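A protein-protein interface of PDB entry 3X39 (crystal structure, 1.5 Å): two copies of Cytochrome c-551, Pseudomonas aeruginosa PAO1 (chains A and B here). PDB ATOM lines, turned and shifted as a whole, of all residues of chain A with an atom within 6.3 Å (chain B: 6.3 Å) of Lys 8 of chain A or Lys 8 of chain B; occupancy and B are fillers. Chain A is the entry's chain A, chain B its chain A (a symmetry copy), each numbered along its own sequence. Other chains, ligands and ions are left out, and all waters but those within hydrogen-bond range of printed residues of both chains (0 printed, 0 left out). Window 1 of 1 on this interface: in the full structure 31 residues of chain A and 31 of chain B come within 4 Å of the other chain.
N of Cys 12 of chain A sits at hydrogen-bond distance from O of Phe 7 of chain A, at 3.4 Å. The backbone NH (N) of Cys 12 of chain B sits at hydrogen-bond distance from the backbone carbonyl oxygen (O) of Phe 7 of chain B, 3.4 Å away.
Phe 7 of chain A touches Val 13 of chain B, and with the chains exchanged Val 13 of chain A touches Phe 7 of chain B. Lys 8 of chain A touches its own counterpart, Lys 8 of chain B. Positions printed for both chains: 3, 4, 5, 6, 7, 8, 9, 10, 11, 12 and 13. Of the 3 pairs that touch across the chains among the printed residues, 3 have their exchanged pair printed and touching as well.
Lys 8 of chain A touches just one residue of chain B: Lys 8 (2.8 Å). Of chain A, only Lys 8 (2.8 Å) comes within 4 Å of Lys 8 of chain B. Printed residues of chain A within 4 Å of Val 13 of chain B: Phe 7 (3.6 Å). Of the printed residues of chain B, Val 13 of chain A touches Phe 7 (3.6 Å). Asn 9 of chain A touches none of the printed residues of chain B. The nearest residue of chain B that does not touch Lys 8 of chain A is Val 13 of chain B (4.3 Å). The nearest printed residue of chain A that does not touch Val 13 of chain B is Lys 8 of chain A (4.3 Å).
O of Lys 8 of chain A is in hydrogen-bond range of NZ of Lys 8 of chain B, 2.8 Å away.
Hydrophobic or aromatic side chains of chain A within 4 Å of the printed part of chain B: Phe 7 and Val 13. Of the 11 printed residues of chain B, 3 touch a printed residue of chain A. Hydrophobic or aromatic side chains of chain B that line the printed part of chain A: Phe 7 and Val 13.
CE1 of Phe 7 of chain A touches CG1 of Val 13 of chain B (3.6 Å). CE1 of Phe 7 of chain B touches CG1 of Val 13 of chain A, at 3.6 Å.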
ATOM      1  N   PRO A   3      21.137 -27.280  -8.124  1.00  0.00           N
ATOM      2  CA  PRO A   3      21.026 -25.862  -8.464  1.00  0.00           C
ATOM      3  C   PRO A   3      19.912 -25.500  -9.418  1.00  0.00           C
ATOM      4  O   PRO A   3      19.363 -24.416  -9.287  1.00  0.00           O
ATOM      5  CB  PRO A   3      22.369 -25.550  -9.117  1.00  0.00           C
ATOM      6  CG  PRO A   3      22.895 -26.869  -9.570  1.00  0.00           C
ATOM      7  CD  PRO A   3      22.450 -27.823  -8.510  1.00  0.00           C
ATOM      8  N   GLU A   4      19.602 -26.351 -10.397  1.00  0.00           N
ATOM      9  CA  GLU A   4      18.463 -26.057 -11.272  1.00  0.00           C
ATOM     10  C   GLU A   4      17.183 -26.042 -10.474  1.00  0.00           C
ATOM     11  O   GLU A   4      16.264 -25.295 -10.793  1.00  0.00           O
ATOM     12  CB  GLU A   4      18.348 -27.046 -12.440  1.00  0.00           C
ATOM     13  CG  GLU A   4      19.341 -26.739 -13.543  1.00  0.00           C
ATOM     14  CD  GLU A   4      19.274 -27.693 -14.715  1.00  0.00           C
ATOM     15  OE1 GLU A   4      18.289 -27.662 -15.498  1.00  0.00           O
ATOM     16  OE2 GLU A   4      20.240 -28.461 -14.860  1.00  0.00           O
ATOM     17  N   VAL A   5      17.119 -26.870  -9.436  1.00  0.00           N
ATOM     18  CA  VAL A   5      15.955 -26.878  -8.575  1.00  0.00           C
ATOM     19  C   VAL A   5      15.858 -25.532  -7.830  1.00  0.00           C
ATOM     20  O   VAL A   5      14.783 -24.951  -7.745  1.00  0.00           O
ATOM     21  CB  VAL A   5      15.972 -28.065  -7.592  1.00  0.00           C
ATOM     22  CG1 VAL A   5      14.845 -27.937  -6.584  1.00  0.00           C
ATOM     23  CG2 VAL A   5      15.828 -29.373  -8.359  1.00  0.00           C
ATOM     24  N   LEU A   6      16.974 -25.046  -7.295  1.00  0.00           N
ATOM     25  CA  LEU A   6      16.973 -23.754  -6.595  1.00  0.00           C
ATOM     26  C   LEU A   6      16.632 -22.588  -7.536  1.00  0.00           C
ATOM     27  O   LEU A   6      15.913 -21.641  -7.164  1.00  0.00           O
ATOM     28  CB  LEU A   6      18.327 -23.510  -5.945  1.00  0.00           C
ATOM     29  CG  LEU A   6      18.691 -24.440  -4.790  1.00  0.00           C
ATOM     30  CD1 LEU A   6      20.154 -24.263  -4.429  1.00  0.00           C
ATOM     31  CD2 LEU A   6      17.797 -24.200  -3.580  1.00  0.00           C
ATOM     32  N   PHE A   7      17.170 -22.647  -8.748  1.00  0.00           N
ATOM     33  CA  PHE A   7      16.914 -21.616  -9.765  1.00  0.00           C
ATOM     34  C   PHE A   7      15.405 -21.378  -9.944  1.00  0.00           C
ATOM     35  O   PHE A   7      14.933 -20.235  -9.997  1.00  0.00           O
ATOM     36  CB  PHE A   7      17.601 -22.043 -11.087  1.00  0.00           C
ATOM     37  CG  PHE A   7      17.292 -21.153 -12.279  1.00  0.00           C
ATOM     38  CD1 PHE A   7      16.665 -21.666 -13.405  1.00  0.00           C
ATOM     39  CD2 PHE A   7      17.668 -19.797 -12.293  1.00  0.00           C
ATOM     40  CE1 PHE A   7      16.394 -20.845 -14.503  1.00  0.00           C
ATOM     41  CE2 PHE A   7      17.394 -18.970 -13.395  1.00  0.00           C
ATOM     42  CZ  PHE A   7      16.752 -19.506 -14.498  1.00  0.00           C
ATOM     43  N   LYS A   8      14.656 -22.478 -10.000  1.00  0.00           N
ATOM     44  CA  LYS A   8      13.208 -22.423 -10.149  1.00  0.00           C
ATOM     45  C   LYS A   8      12.539 -22.053  -8.819  1.00  0.00           C
ATOM     46  O   LYS A   8      11.685 -21.163  -8.775  1.00  0.00           O
ATOM     47  CB  LYS A   8      12.683 -23.754 -10.708  1.00  0.00           C
ATOM     48  CG  LYS A   8      13.414 -24.210 -11.971  1.00  0.00           C
ATOM     49  CD  LYS A   8      12.630 -25.216 -12.803  1.00  0.00           C
ATOM     50  CE  LYS A   8      12.578 -26.599 -12.183  1.00  0.00           C
ATOM     51  NZ  LYS A   8      12.128 -27.593 -13.202  1.00  0.00           N
ATOM     52  N   ASN A   9      12.948 -22.697  -7.729  1.00  0.00           N
ATOM     53  CA  ASN A   9      12.237 -22.554  -6.455  1.00  0.00           C
ATOM     54  C   ASN A   9      12.478 -21.213  -5.788  1.00  0.00           C
ATOM     55  O   ASN A   9      11.626 -20.742  -5.029  1.00  0.00           O
ATOM     56  CB  ASN A   9      12.642 -23.651  -5.468  1.00  0.00           C
ATOM     57  CG  ASN A   9      12.083 -25.012  -5.826  1.00  0.00           C
ATOM     58  OD1 ASN A   9      11.459 -25.212  -6.880  1.00  0.00           O
ATOM     59  ND2 ASN A   9      12.311 -25.969  -4.939  1.00  0.00           N
ATOM     60  N   LYS A  10      13.630 -20.598  -6.056  1.00  0.00           N
ATOM     61  CA  LYS A  10      13.993 -19.347  -5.367  1.00  0.00           C
ATOM     62  C   LYS A  10      13.747 -18.061  -6.157  1.00  0.00           C
ATOM     63  O   LYS A  10      14.252 -16.975  -5.774  1.00  0.00           O
ATOM     64  CB  LYS A  10      15.449 -19.406  -4.891  1.00  0.00           C
ATOM     65  CG  LYS A  10      15.783 -20.592  -4.005  1.00  0.00           C
ATOM     66  CD  LYS A  10      14.974 -20.520  -2.719  1.00  0.00           C
ATOM     67  CE  LYS A  10      15.398 -21.592  -1.746  1.00  0.00           C
ATOM     68  NZ  LYS A  10      14.654 -21.466  -0.462  1.00  0.00           N
ATOM     69  N   GLY A  11      12.956 -18.154  -7.231  1.00  0.00           N
ATOM     70  CA  GLY A  11      12.457 -16.963  -7.927  1.00  0.00           C
ATOM     71  C   GLY A  11      13.361 -16.332  -8.984  1.00  0.00           C
ATOM     72  O   GLY A  11      13.014 -15.326  -9.603  1.00  0.00           O
ATOM     73  N   CYS A  12      14.492 -16.968  -9.243  1.00  0.00           N
ATOM     74  CA  CYS A  12      15.500 -16.427 -10.142  1.00  0.00           C
ATOM     75  C   CYS A  12      14.983 -16.341 -11.571  1.00  0.00           C
ATOM     76  O   CYS A  12      15.392 -15.468 -12.331  1.00  0.00           O
ATOM     77  CB  CYS A  12      16.722 -17.339 -10.146  1.00  0.00           C
ATOM     78  SG  CYS A  12      17.278 -17.912  -8.533  1.00  0.00           S
ATOM     79  N   VAL A  13      14.101 -17.285 -11.922  1.00  0.00           N
ATOM     80  CA  VAL A  13      13.542 -17.397 -13.284  1.00  0.00           C
ATOM     81  C   VAL A  13      12.791 -16.141 -13.735  1.00  0.00           C
ATOM     82  O   VAL A  13      12.690 -15.888 -14.937  1.00  0.00           O
ATOM     83  CB  VAL A  13      12.590 -18.622 -13.388  1.00  0.00           C
ATOM     84  CG1 VAL A  13      11.967 -18.719 -14.778  1.00  0.00           C
ATOM     85  CG2 VAL A  13      13.334 -19.902 -13.097  1.00  0.00           C
ATOM     86  N   PRO B   3       0.198 -20.591 -14.673  1.00  0.00           N
ATOM     87  CA  PRO B   3       1.107 -20.919 -15.771  1.00  0.00           C
ATOM     88  C   PRO B   3       2.580 -20.789 -15.465  1.00  0.00           C
ATOM     89  O   PRO B   3       3.358 -21.563 -16.007  1.00  0.00           O
ATOM     90  CB  PRO B   3       0.728 -19.915 -16.855  1.00  0.00           C
ATOM     91  CG  PRO B   3       0.051 -18.802 -16.130  1.00  0.00           C
ATOM     92  CD  PRO B   3      -0.701 -19.483 -15.034  1.00  0.00           C
ATOM     93  N   GLU B   4       2.986 -19.809 -14.657  1.00  0.00           N
ATOM     94  CA  GLU B   4       4.399 -19.728 -14.277  1.00  0.00           C
ATOM     95  C   GLU B   4       4.796 -20.949 -13.485  1.00  0.00           C
ATOM     96  O   GLU B   4       5.938 -21.393 -13.566  1.00  0.00           O
ATOM     97  CB  GLU B   4       4.724 -18.453 -13.486  1.00  0.00           C
ATOM     98  CG  GLU B   4       4.842 -17.241 -14.386  1.00  0.00           C
ATOM     99  CD  GLU B   4       5.152 -15.956 -13.651  1.00  0.00           C
ATOM    100  OE1 GLU B   4       6.290 -15.777 -13.144  1.00  0.00           O
ATOM    101  OE2 GLU B   4       4.244 -15.107 -13.611  1.00  0.00           O
ATOM    102  N   VAL B   5       3.858 -21.491 -12.716  1.00  0.00           N
ATOM    103  CA  VAL B   5       4.130 -22.702 -11.970  1.00  0.00           C
ATOM    104  C   VAL B   5       4.358 -23.869 -12.951  1.00  0.00           C
ATOM    105  O   VAL B   5       5.291 -24.643 -12.780  1.00  0.00           O
ATOM    106  CB  VAL B   5       3.009 -23.024 -10.964  1.00  0.00           C
ATOM    107  CG1 VAL B   5       3.230 -24.389 -10.340  1.00  0.00           C
ATOM    108  CG2 VAL B   5       2.973 -21.962  -9.872  1.00  0.00           C
ATOM    109  N   LEU B   6       3.509 -23.990 -13.968  1.00  0.00           N
ATOM    110  CA  LEU B   6       3.674 -25.057 -14.964  1.00  0.00           C
ATOM    111  C   LEU B   6       4.980 -24.906 -15.761  1.00  0.00           C
ATOM    112  O   LEU B   6       5.668 -25.895 -16.076  1.00  0.00           O
ATOM    113  CB  LEU B   6       2.489 -25.070 -15.918  1.00  0.00           C
ATOM    114  CG  LEU B   6       1.148 -25.476 -15.313  1.00  0.00           C
ATOM    115  CD1 LEU B   6       0.030 -25.181 -16.295  1.00  0.00           C
ATOM    116  CD2 LEU B   6       1.144 -26.944 -14.904  1.00  0.00           C
ATOM    117  N   PHE B   7       5.306 -23.666 -16.106  1.00  0.00           N
ATOM    118  CA  PHE B   7       6.539 -23.362 -16.848  1.00  0.00           C
ATOM    119  C   PHE B   7       7.766 -23.986 -16.161  1.00  0.00           C
ATOM    120  O   PHE B   7       8.625 -24.598 -16.807  1.00  0.00           O
ATOM    121  CB  PHE B   7       6.665 -21.823 -16.991  1.00  0.00           C
ATOM    122  CG  PHE B   7       7.973 -21.348 -17.600  1.00  0.00           C
ATOM    123  CD1 PHE B   7       8.829 -20.522 -16.887  1.00  0.00           C
ATOM    124  CD2 PHE B   7       8.335 -21.697 -18.915  1.00  0.00           C
ATOM    125  CE1 PHE B   7      10.026 -20.078 -17.457  1.00  0.00           C
ATOM    126  CE2 PHE B   7       9.538 -21.253 -19.488  1.00  0.00           C
ATOM    127  CZ  PHE B   7      10.381 -20.443 -18.745  1.00  0.00           C
ATOM    128  N   LYS B   8       7.812 -23.847 -14.837  1.00  0.00           N
ATOM    129  CA  LYS B   8       8.898 -24.395 -14.038  1.00  0.00           C
ATOM    130  C   LYS B   8       8.729 -25.910 -13.858  1.00  0.00           C
ATOM    131  O   LYS B   8       9.676 -26.673 -14.069  1.00  0.00           O
ATOM    132  CB  LYS B   8       8.985 -23.662 -12.690  1.00  0.00           C
ATOM    133  CG  LYS B   8       9.035 -22.140 -12.832  1.00  0.00           C
ATOM    134  CD  LYS B   8       9.603 -21.430 -11.612  1.00  0.00           C
ATOM    135  CE  LYS B   8       8.653 -21.414 -10.428  1.00  0.00           C
ATOM    136  NZ  LYS B   8       9.114 -20.408  -9.426  1.00  0.00           N
ATOM    137  N   ASN B   9       7.524 -26.354 -13.514  1.00  0.00           N
ATOM    138  CA  ASN B   9       7.315 -27.753 -13.131  1.00  0.00           C
ATOM    139  C   ASN B   9       7.359 -28.705 -14.311  1.00  0.00           C
ATOM    140  O   ASN B   9       7.696 -29.880 -14.141  1.00  0.00           O
ATOM    141  CB  ASN B   9       5.970 -27.941 -12.425  1.00  0.00           C
ATOM    142  CG  ASN B   9       5.949 -27.373 -11.021  1.00  0.00           C
ATOM    143  OD1 ASN B   9       6.901 -26.725 -10.558  1.00  0.00           O
ATOM    144  ND2 ASN B   9       4.846 -27.613 -10.329  1.00  0.00           N
ATOM    145  N   LYS B  10       7.018 -28.214 -15.502  1.00  0.00           N
ATOM    146  CA  LYS B  10       6.926 -29.093 -16.681  1.00  0.00           C
ATOM    147  C   LYS B  10       8.133 -29.068 -17.621  1.00  0.00           C
ATOM    148  O   LYS B  10       8.053 -29.573 -18.770  1.00  0.00           O
ATOM    149  CB  LYS B  10       5.639 -28.802 -17.463  1.00  0.00           C
ATOM    150  CG  LYS B  10       4.363 -28.906 -16.649  1.00  0.00           C
ATOM    151  CD  LYS B  10       4.181 -30.332 -16.150  1.00  0.00           C
ATOM    152  CE  LYS B  10       2.843 -30.508 -15.476  1.00  0.00           C
ATOM    153  NZ  LYS B  10       2.643 -31.924 -15.060  1.00  0.00           N
ATOM    154  N   GLY B  11       9.256 -28.520 -17.146  1.00  0.00           N
ATOM    155  CA  GLY B  11      10.535 -28.646 -17.855  1.00  0.00           C
ATOM    156  C   GLY B  11      10.831 -27.636 -18.962  1.00  0.00           C
ATOM    157  O   GLY B  11      11.879 -27.683 -19.605  1.00  0.00           O
ATOM    158  N   CYS B  12       9.938 -26.674 -19.131  1.00  0.00           N
ATOM    159  CA  CYS B  12      10.032 -25.709 -20.217  1.00  0.00           C
ATOM    160  C   CYS B  12      11.261 -24.824 -20.071  1.00  0.00           C
ATOM    161  O   CYS B  12      11.824 -24.368 -21.062  1.00  0.00           O
ATOM    162  CB  CYS B  12       8.804 -24.806 -20.203  1.00  0.00           C
ATOM    163  SG  CYS B  12       7.224 -25.633 -19.969  1.00  0.00           S
ATOM    164  N   VAL B  13      11.639 -24.567 -18.813  1.00  0.00           N
ATOM    165  CA  VAL B  13      12.768 -23.677 -18.477  1.00  0.00           C
ATOM    166  C   VAL B  13      14.101 -24.138 -19.074  1.00  0.00           C
ATOM    167  O   VAL B  13      14.990 -23.314 -19.292  1.00  0.00           O
ATOM    168  CB  VAL B  13      12.922 -23.542 -16.935  1.00  0.00           C
ATOM    169  CG1 VAL B  13      14.116 -22.664 -16.576  1.00  0.00           C
ATOM    170  CG2 VAL B  13      11.678 -22.946 -16.324  1.00  0.00           C
